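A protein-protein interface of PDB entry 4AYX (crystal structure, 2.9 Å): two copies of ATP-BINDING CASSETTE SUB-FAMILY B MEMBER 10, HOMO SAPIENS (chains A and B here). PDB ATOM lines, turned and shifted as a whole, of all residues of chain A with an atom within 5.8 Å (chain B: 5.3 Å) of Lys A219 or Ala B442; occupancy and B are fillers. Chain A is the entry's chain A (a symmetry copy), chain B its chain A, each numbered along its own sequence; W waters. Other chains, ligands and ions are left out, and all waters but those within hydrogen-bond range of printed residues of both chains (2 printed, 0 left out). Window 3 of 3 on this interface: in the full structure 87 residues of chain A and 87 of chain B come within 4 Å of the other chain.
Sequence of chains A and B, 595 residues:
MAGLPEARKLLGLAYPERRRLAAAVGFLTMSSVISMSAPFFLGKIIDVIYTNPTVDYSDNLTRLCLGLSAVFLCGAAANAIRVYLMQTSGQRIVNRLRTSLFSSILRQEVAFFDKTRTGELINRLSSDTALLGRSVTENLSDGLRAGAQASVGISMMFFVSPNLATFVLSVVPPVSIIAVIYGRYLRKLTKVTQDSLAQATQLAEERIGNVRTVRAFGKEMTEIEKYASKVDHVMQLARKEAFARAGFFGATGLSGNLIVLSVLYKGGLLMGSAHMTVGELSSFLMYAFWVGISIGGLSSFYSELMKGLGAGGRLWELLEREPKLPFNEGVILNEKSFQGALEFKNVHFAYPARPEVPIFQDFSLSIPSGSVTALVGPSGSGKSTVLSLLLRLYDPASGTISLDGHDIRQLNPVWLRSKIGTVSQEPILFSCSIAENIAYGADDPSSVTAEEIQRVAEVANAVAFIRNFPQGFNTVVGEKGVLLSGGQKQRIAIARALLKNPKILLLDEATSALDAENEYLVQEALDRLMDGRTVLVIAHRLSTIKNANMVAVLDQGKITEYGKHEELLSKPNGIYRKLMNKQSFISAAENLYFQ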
ATOM      1  N   VAL A 214     -20.163   7.927  22.450  1.00  0.00           N
ATOM      2  CA  VAL A 214     -19.219   9.051  22.447  1.00  0.00           C
ATOM      3  C   VAL A 214     -17.837   8.567  23.012  1.00  0.00           C
ATOM      4  O   VAL A 214     -16.821   8.840  22.379  1.00  0.00           O
ATOM      5  CB  VAL A 214     -19.792  10.279  23.218  1.00  0.00           C
ATOM      6  CG1 VAL A 214     -18.746  11.368  23.390  1.00  0.00           C
ATOM      7  CG2 VAL A 214     -21.037  10.839  22.526  1.00  0.00           C
ATOM      8  N   ARG A 215     -17.814   7.830  24.165  1.00  0.00           N
ATOM      9  CA  ARG A 215     -16.595   7.282  24.772  1.00  0.00           C
ATOM     10  C   ARG A 215     -15.904   6.370  23.812  1.00  0.00           C
ATOM     11  O   ARG A 215     -14.696   6.522  23.597  1.00  0.00           O
ATOM     12  CB  ARG A 215     -16.880   6.477  26.058  1.00  0.00           C
ATOM     13  CG  ARG A 215     -17.220   7.309  27.251  1.00  0.00           C
ATOM     14  CD  ARG A 215     -16.399   6.991  28.494  1.00  0.00           C
ATOM     15  NE  ARG A 215     -15.986   8.250  29.121  1.00  0.00           N
ATOM     16  CZ  ARG A 215     -16.771   9.029  29.861  1.00  0.00           C
ATOM     17  NH1 ARG A 215     -17.997   8.645  30.173  1.00  0.00           N
ATOM     18  NH2 ARG A 215     -16.321  10.179  30.330  1.00  0.00           N
ATOM     19  N   PHE A 217     -15.761   6.136  20.686  1.00  0.00           N
ATOM     20  CA  PHE A 217     -15.049   6.811  19.608  1.00  0.00           C
ATOM     21  C   PHE A 217     -14.160   7.981  20.108  1.00  0.00           C
ATOM     22  O   PHE A 217     -13.700   8.786  19.290  1.00  0.00           O
ATOM     23  CB  PHE A 217     -16.063   7.303  18.556  1.00  0.00           C
ATOM     24  CG  PHE A 217     -16.721   6.148  17.842  1.00  0.00           C
ATOM     25  CD1 PHE A 217     -16.114   5.552  16.744  1.00  0.00           C
ATOM     26  CD2 PHE A 217     -17.910   5.605  18.312  1.00  0.00           C
ATOM     27  CE1 PHE A 217     -16.680   4.436  16.133  1.00  0.00           C
ATOM     28  CE2 PHE A 217     -18.485   4.501  17.689  1.00  0.00           C
ATOM     29  CZ  PHE A 217     -17.870   3.927  16.601  1.00  0.00           C
ATOM     30  N   GLY A 218     -13.902   8.033  21.425  1.00  0.00           N
ATOM     31  CA  GLY A 218     -13.102   9.063  22.081  1.00  0.00           C
ATOM     32  C   GLY A 218     -13.440  10.446  21.569  1.00  0.00           C
ATOM     33  O   GLY A 218     -12.551  11.159  21.098  1.00  0.00           O
ATOM     34  N   LYS A 219     -14.743  10.798  21.583  1.00  0.00           N
ATOM     35  CA  LYS A 219     -15.222  12.073  21.053  1.00  0.00           C
ATOM     36  C   LYS A 219     -15.750  13.045  22.138  1.00  0.00           C
ATOM     37  O   LYS A 219     -16.334  14.070  21.790  1.00  0.00           O
ATOM     38  CB  LYS A 219     -16.308  11.820  19.998  1.00  0.00           C
ATOM     39  CG  LYS A 219     -15.801  11.180  18.711  1.00  0.00           C
ATOM     40  CD  LYS A 219     -14.980  12.144  17.852  1.00  0.00           C
ATOM     41  CE  LYS A 219     -14.296  11.452  16.702  1.00  0.00           C
ATOM     42  NZ  LYS A 219     -13.135  10.629  17.135  1.00  0.00           N
ATOM     43  N   GLU A 220     -15.503  12.765  23.433  1.00  0.00           N
ATOM     44  CA  GLU A 220     -15.957  13.645  24.514  1.00  0.00           C
ATOM     45  C   GLU A 220     -15.457  15.053  24.299  1.00  0.00           C
ATOM     46  O   GLU A 220     -16.284  15.952  24.241  1.00  0.00           O
ATOM     47  CB  GLU A 220     -15.539  13.137  25.900  1.00  0.00           C
ATOM     48  CG  GLU A 220     -16.080  11.769  26.270  1.00  0.00           C
ATOM     49  CD  GLU A 220     -15.009  10.700  26.297  1.00  0.00           C
ATOM     50  OE1 GLU A 220     -14.254  10.587  25.303  1.00  0.00           O
ATOM     51  OE2 GLU A 220     -14.884  10.017  27.339  1.00  0.00           O
ATOM     52  N   MET A 221     -14.130  15.244  24.103  1.00  0.00           N
ATOM     53  CA  MET A 221     -13.502  16.552  23.873  1.00  0.00           C
ATOM     54  C   MET A 221     -14.036  17.238  22.615  1.00  0.00           C
ATOM     55  O   MET A 221     -14.190  18.461  22.606  1.00  0.00           O
ATOM     56  CB  MET A 221     -11.975  16.446  23.791  1.00  0.00           C
ATOM     57  CG  MET A 221     -11.273  16.379  25.133  1.00  0.00           C
ATOM     58  SD  MET A 221     -11.863  17.512  26.441  1.00  0.00           S
ATOM     59  CE  MET A 221     -11.667  19.173  25.645  1.00  0.00           C
ATOM     60  N   THR A 222     -14.346  16.446  21.577  1.00  0.00           N
ATOM     61  CA  THR A 222     -14.893  16.918  20.303  1.00  0.00           C
ATOM     62  C   THR A 222     -16.316  17.498  20.509  1.00  0.00           C
ATOM     63  O   THR A 222     -16.579  18.611  20.041  1.00  0.00           O
ATOM     64  CB  THR A 222     -14.862  15.776  19.270  1.00  0.00           C
ATOM     65  OG1 THR A 222     -13.515  15.303  19.160  1.00  0.00           O
ATOM     66  CG2 THR A 222     -15.376  16.203  17.898  1.00  0.00           C
ATOM     67  N   GLU A 223     -17.208  16.746  21.212  1.00  0.00           N
ATOM     68  CA  GLU A 223     -18.593  17.134  21.513  1.00  0.00           C
ATOM     69  C   GLU A 223     -18.638  18.344  22.416  1.00  0.00           C
ATOM     70  O   GLU A 223     -19.427  19.249  22.160  1.00  0.00           O
ATOM     71  CB  GLU A 223     -19.386  15.987  22.152  1.00  0.00           C
ATOM     72  CG  GLU A 223     -19.525  14.735  21.293  1.00  0.00           C
ATOM     73  CD  GLU A 223     -20.204  14.822  19.937  1.00  0.00           C
ATOM     74  OE1 GLU A 223     -20.576  15.929  19.483  1.00  0.00           O
ATOM     75  OE2 GLU A 223     -20.385  13.745  19.331  1.00  0.00           O
ATOM     76  N   ILE A 224     -17.779  18.374  23.462  1.00  0.00           N
ATOM     77  CA  ILE A 224     -17.651  19.485  24.402  1.00  0.00           C
ATOM     78  C   ILE A 224     -17.412  20.783  23.599  1.00  0.00           C
ATOM     79  O   ILE A 224     -18.125  21.762  23.802  1.00  0.00           O
ATOM     80  CB  ILE A 224     -16.523  19.194  25.440  1.00  0.00           C
ATOM     81  CG1 ILE A 224     -16.975  18.115  26.456  1.00  0.00           C
ATOM     82  CG2 ILE A 224     -16.066  20.475  26.153  1.00  0.00           C
ATOM     83  CD1 ILE A 224     -15.856  17.462  27.289  1.00  0.00           C
ATOM     84  N   ILE B 438     -20.297   8.830   9.660  1.00  0.00           N
ATOM     85  CA  ILE B 438     -19.207   7.966   9.198  1.00  0.00           C
ATOM     86  C   ILE B 438     -17.861   8.559   9.677  1.00  0.00           C
ATOM     87  O   ILE B 438     -17.036   7.824  10.222  1.00  0.00           O
ATOM     88  CB  ILE B 438     -19.254   7.752   7.649  1.00  0.00           C
ATOM     89  CG1 ILE B 438     -20.493   6.916   7.236  1.00  0.00           C
ATOM     90  CG2 ILE B 438     -17.949   7.108   7.114  1.00  0.00           C
ATOM     91  CD1 ILE B 438     -20.884   7.010   5.749  1.00  0.00           C
ATOM     92  N   ALA B 439     -17.667   9.887   9.498  1.00  0.00           N
ATOM     93  CA  ALA B 439     -16.460  10.632   9.873  1.00  0.00           C
ATOM     94  C   ALA B 439     -16.103  10.471  11.359  1.00  0.00           C
ATOM     95  O   ALA B 439     -14.927  10.566  11.712  1.00  0.00           O
ATOM     96  CB  ALA B 439     -16.629  12.102   9.540  1.00  0.00           C
ATOM     97  N   TYR B 440     -17.112  10.174  12.208  1.00  0.00           N
ATOM     98  CA  TYR B 440     -17.015   9.949  13.656  1.00  0.00           C
ATOM     99  C   TYR B 440     -15.981   8.871  14.035  1.00  0.00           C
ATOM    100  O   TYR B 440     -15.509   8.862  15.177  1.00  0.00           O
ATOM    101  CB  TYR B 440     -18.386   9.535  14.197  1.00  0.00           C
ATOM    102  CG  TYR B 440     -18.647   9.984  15.611  1.00  0.00           C
ATOM    103  CD1 TYR B 440     -18.858  11.326  15.908  1.00  0.00           C
ATOM    104  CD2 TYR B 440     -18.756   9.060  16.647  1.00  0.00           C
ATOM    105  CE1 TYR B 440     -19.124  11.747  17.209  1.00  0.00           C
ATOM    106  CE2 TYR B 440     -19.025   9.469  17.953  1.00  0.00           C
ATOM    107  CZ  TYR B 440     -19.228  10.814  18.224  1.00  0.00           C
ATOM    108  OH  TYR B 440     -19.501  11.250  19.492  1.00  0.00           O
ATOM    109  N   GLY B 441     -15.659   7.977  13.095  1.00  0.00           N
ATOM    110  CA  GLY B 441     -14.673   6.925  13.297  1.00  0.00           C
ATOM    111  C   GLY B 441     -13.265   7.471  13.461  1.00  0.00           C
ATOM    112  O   GLY B 441     -12.529   7.035  14.350  1.00  0.00           O
ATOM    113  N   ALA B 442     -12.900   8.457  12.614  1.00  0.00           N
ATOM    114  CA  ALA B 442     -11.590   9.115  12.562  1.00  0.00           C
ATOM    115  C   ALA B 442     -11.243   9.850  13.850  1.00  0.00           C
ATOM    116  O   ALA B 442     -12.134  10.385  14.506  1.00  0.00           O
ATOM    117  CB  ALA B 442     -11.561  10.097  11.405  1.00  0.00           C
ATOM    118  N   ASP B 443      -9.935   9.921  14.183  1.00  0.00           N
ATOM    119  CA  ASP B 443      -9.436  10.641  15.367  1.00  0.00           C
ATOM    120  C   ASP B 443      -9.621  12.168  15.190  1.00  0.00           C
ATOM    121  O   ASP B 443      -9.683  12.910  16.177  1.00  0.00           O
ATOM    122  CB  ASP B 443      -7.967  10.276  15.659  1.00  0.00           C
ATOM    123  CG  ASP B 443      -7.725   8.808  16.018  1.00  0.00           C
ATOM    124  OD1 ASP B 443      -8.697   8.119  16.434  1.00  0.00           O
ATOM    125  OD2 ASP B 443      -6.560   8.354  15.909  1.00  0.00           O
ATOM    126  N   ASP B 444      -9.747  12.616  13.923  1.00  0.00           N
ATOM    127  CA  ASP B 444     -10.030  13.991  13.526  1.00  0.00           C
ATOM    128  C   ASP B 444     -11.122  13.939  12.442  1.00  0.00           C
ATOM    129  O   ASP B 444     -10.793  13.897  11.252  1.00  0.00           O
ATOM    130  CB  ASP B 444      -8.755  14.725  13.053  1.00  0.00           C
ATOM    131  CG  ASP B 444      -8.886  16.237  12.883  1.00  0.00           C
ATOM    132  OD1 ASP B 444      -9.907  16.808  13.345  1.00  0.00           O
ATOM    133  OD2 ASP B 444      -7.953  16.856  12.319  1.00  0.00           O
ATOM    134  N   PRO B 445     -12.427  13.902  12.832  1.00  0.00           N
ATOM    135  CA  PRO B 445     -13.504  13.797  11.822  1.00  0.00           C
ATOM    136  C   PRO B 445     -13.604  15.003  10.873  1.00  0.00           C
ATOM    137  O   PRO B 445     -14.373  14.951   9.911  1.00  0.00           O
ATOM    138  CB  PRO B 445     -14.774  13.647  12.667  1.00  0.00           C
ATOM    139  CG  PRO B 445     -14.428  14.183  13.993  1.00  0.00           C
ATOM    140  CD  PRO B 445     -12.979  13.916  14.202  1.00  0.00           C
ATOM    141  N   VAL B 448     -10.875  14.205   7.630  1.00  0.00           N
ATOM    142  CA  VAL B 448     -11.273  13.233   6.599  1.00  0.00           C
ATOM    143  C   VAL B 448     -11.935  13.922   5.408  1.00  0.00           C
ATOM    144  O   VAL B 448     -12.785  14.802   5.571  1.00  0.00           O
ATOM    145  CB  VAL B 448     -12.140  12.051   7.108  1.00  0.00           C
ATOM    146  CG1 VAL B 448     -11.282  11.009   7.812  1.00  0.00           C
ATOM    147  CG2 VAL B 448     -13.278  12.519   8.004  1.00  0.00           C
ATOM    148  N   ARG B 496     -18.040   3.406   9.694  1.00  0.00           N
ATOM    149  CA  ARG B 496     -17.454   4.141  10.808  1.00  0.00           C
ATOM    150  C   ARG B 496     -16.261   3.340  11.410  1.00  0.00           C
ATOM    151  O   ARG B 496     -15.218   3.932  11.701  1.00  0.00           O
ATOM    152  CB  ARG B 496     -18.539   4.417  11.850  1.00  0.00           C
ATOM    153  CG  ARG B 496     -18.115   5.363  12.962  1.00  0.00           C
ATOM    154  CD  ARG B 496     -19.303   5.895  13.742  1.00  0.00           C
ATOM    155  NE  ARG B 496     -20.139   4.849  14.334  1.00  0.00           N
ATOM    156  CZ  ARG B 496     -21.355   5.060  14.833  1.00  0.00           C
ATOM    157  NH1 ARG B 496     -21.895   6.275  14.800  1.00  0.00           N
ATOM    158  NH2 ARG B 496     -22.043   4.055  15.361  1.00  0.00           N
ATOM    159  N   LEU B 499     -13.218   3.321   8.836  1.00  0.00           N
ATOM    160  CA  LEU B 499     -12.519   4.604   8.890  1.00  0.00           C
ATOM    161  C   LEU B 499     -11.670   4.704  10.154  1.00  0.00           C
ATOM    162  O   LEU B 499     -10.568   5.249  10.093  1.00  0.00           O
ATOM    163  CB  LEU B 499     -13.515   5.770   8.824  1.00  0.00           C
ATOM    164  CG  LEU B 499     -12.932   7.141   8.498  1.00  0.00           C
ATOM    165  CD1 LEU B 499     -12.729   7.318   6.993  1.00  0.00           C
ATOM    166  CD2 LEU B 499     -13.830   8.226   9.012  1.00  0.00           C
ATOM    167  N   LYS B 500     -12.171   4.162  11.292  1.00  0.00           N
ATOM    168  CA  LYS B 500     -11.424   4.130  12.551  1.00  0.00           C
ATOM    169  C   LYS B 500     -10.173   3.271  12.362  1.00  0.00           C
ATOM    170  O   LYS B 500      -9.101   3.651  12.834  1.00  0.00           O
ATOM    171  CB  LYS B 500     -12.288   3.587  13.709  1.00  0.00           C
ATOM    172  CG  LYS B 500     -11.613   3.724  15.070  1.00  0.00           C
ATOM    173  CD  LYS B 500     -12.171   2.776  16.120  1.00  0.00           C
ATOM    174  CE  LYS B 500     -12.976   3.485  17.186  1.00  0.00           C
ATOM    175  NZ  LYS B 500     -12.140   4.360  18.050  1.00  0.00           N
HETATM  176  O   HOH W   1     -12.272   7.117  17.052  1.00  0.00           O
HETATM  177  O   HOH W   2     -10.469  11.959  18.360  1.00  0.00           O
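OE2 of Glu A223 lies within hydrogen-bond range of OH of Tyr B440 (2.7 Å).
The backbone carbonyl oxygen (O) of Ala B442 sits at hydrogen-bond distance from the side-chain amino group (NZ) of Lys A219, 2.8 Å away.
Tyr B440 touches Val A214.
CD1 of Phe A217 touches O of Tyr B440, at 3.7 Å.
Gly B441 touches Phe A217 (CA to CD1, 3.98 Å).
CZ of Phe A217 touches NE of Arg B496, 3.3 Å away.
CE of Lys B500 touches CD1 of Phe A217 (3.8 Å).
Lys A219 touches Tyr B440 (CE to O, 3.2 Å).
CE of Lys A219 touches CD of Pro B445, at 3.7 Å.
Water W2 lies within hydrogen-bond range of O of Asp B443 (2.5 Å) and NZ of Lys A219 (3.2 Å).
Water W1 lies within hydrogen-bond range of O of Gly B441 (2.7 Å), NZ of Lys B500 (2.9 Å) and O of Phe A217 (3.1 Å).
O of Val A214 sits at hydrogen-bond distance from N of Lys A219.
O of Phe A217 lies within hydrogen-bond range of NZ of Lys A219, at 2.9 Å.
Printed residues of chain B that touch a printed residue of chain A: Tyr B440, Gly B441, Ala B442, Pro B445, Arg B496 and Lys B500.
Hydrophobic or aromatic side chains of chain B within 4 Å of the printed part of chain A: Tyr B440 and Pro B445.
Hydrophobic or aromatic side chains of chain A within 4 Å of the printed part of chain B: Val A214 and Phe A217.
Among the printed residues, 9 pairs touch across the chains.
Among the printed residues, no Asp or Glu carboxylate lies within 4 Å of a Lys or Arg side-chain nitrogen of the other chain.
Printed residues of chain B within 4 Å of Phe A217: Tyr B440 (3.7 Å), Gly B441 (3.98 Å), Arg B496 (3.3 Å) and Lys B500 (3.8 Å).
Of chain B, only Tyr B440 (3.2 Å), Ala B442 (2.8 Å) and Pro B445 (3.7 Å) come within 4 Å of Lys A219.
Ala B439 touches none of the printed residues of chain A.
Printed residues of chain A within 4 Å of Gly B441: Phe A217 (3.98 Å).
Of the printed residues of chain A, Ala B442 touches Lys A219.
Of the printed residues of chain A, Pro B445 touches Lys A219.
Printed residues of chain A within 4 Å of Arg B496: Phe A217 (3.3 Å).
Of the printed residues of chain A, Lys B500 touches Phe A217.
The nearest printed residue of chain B that does not touch Val A214 is Lys B500 (7.8 Å).
No position is printed for both chains.
Of the 9 pairs that touch across the chains among the printed residues, none has its exchanged pair printed and touching as well.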
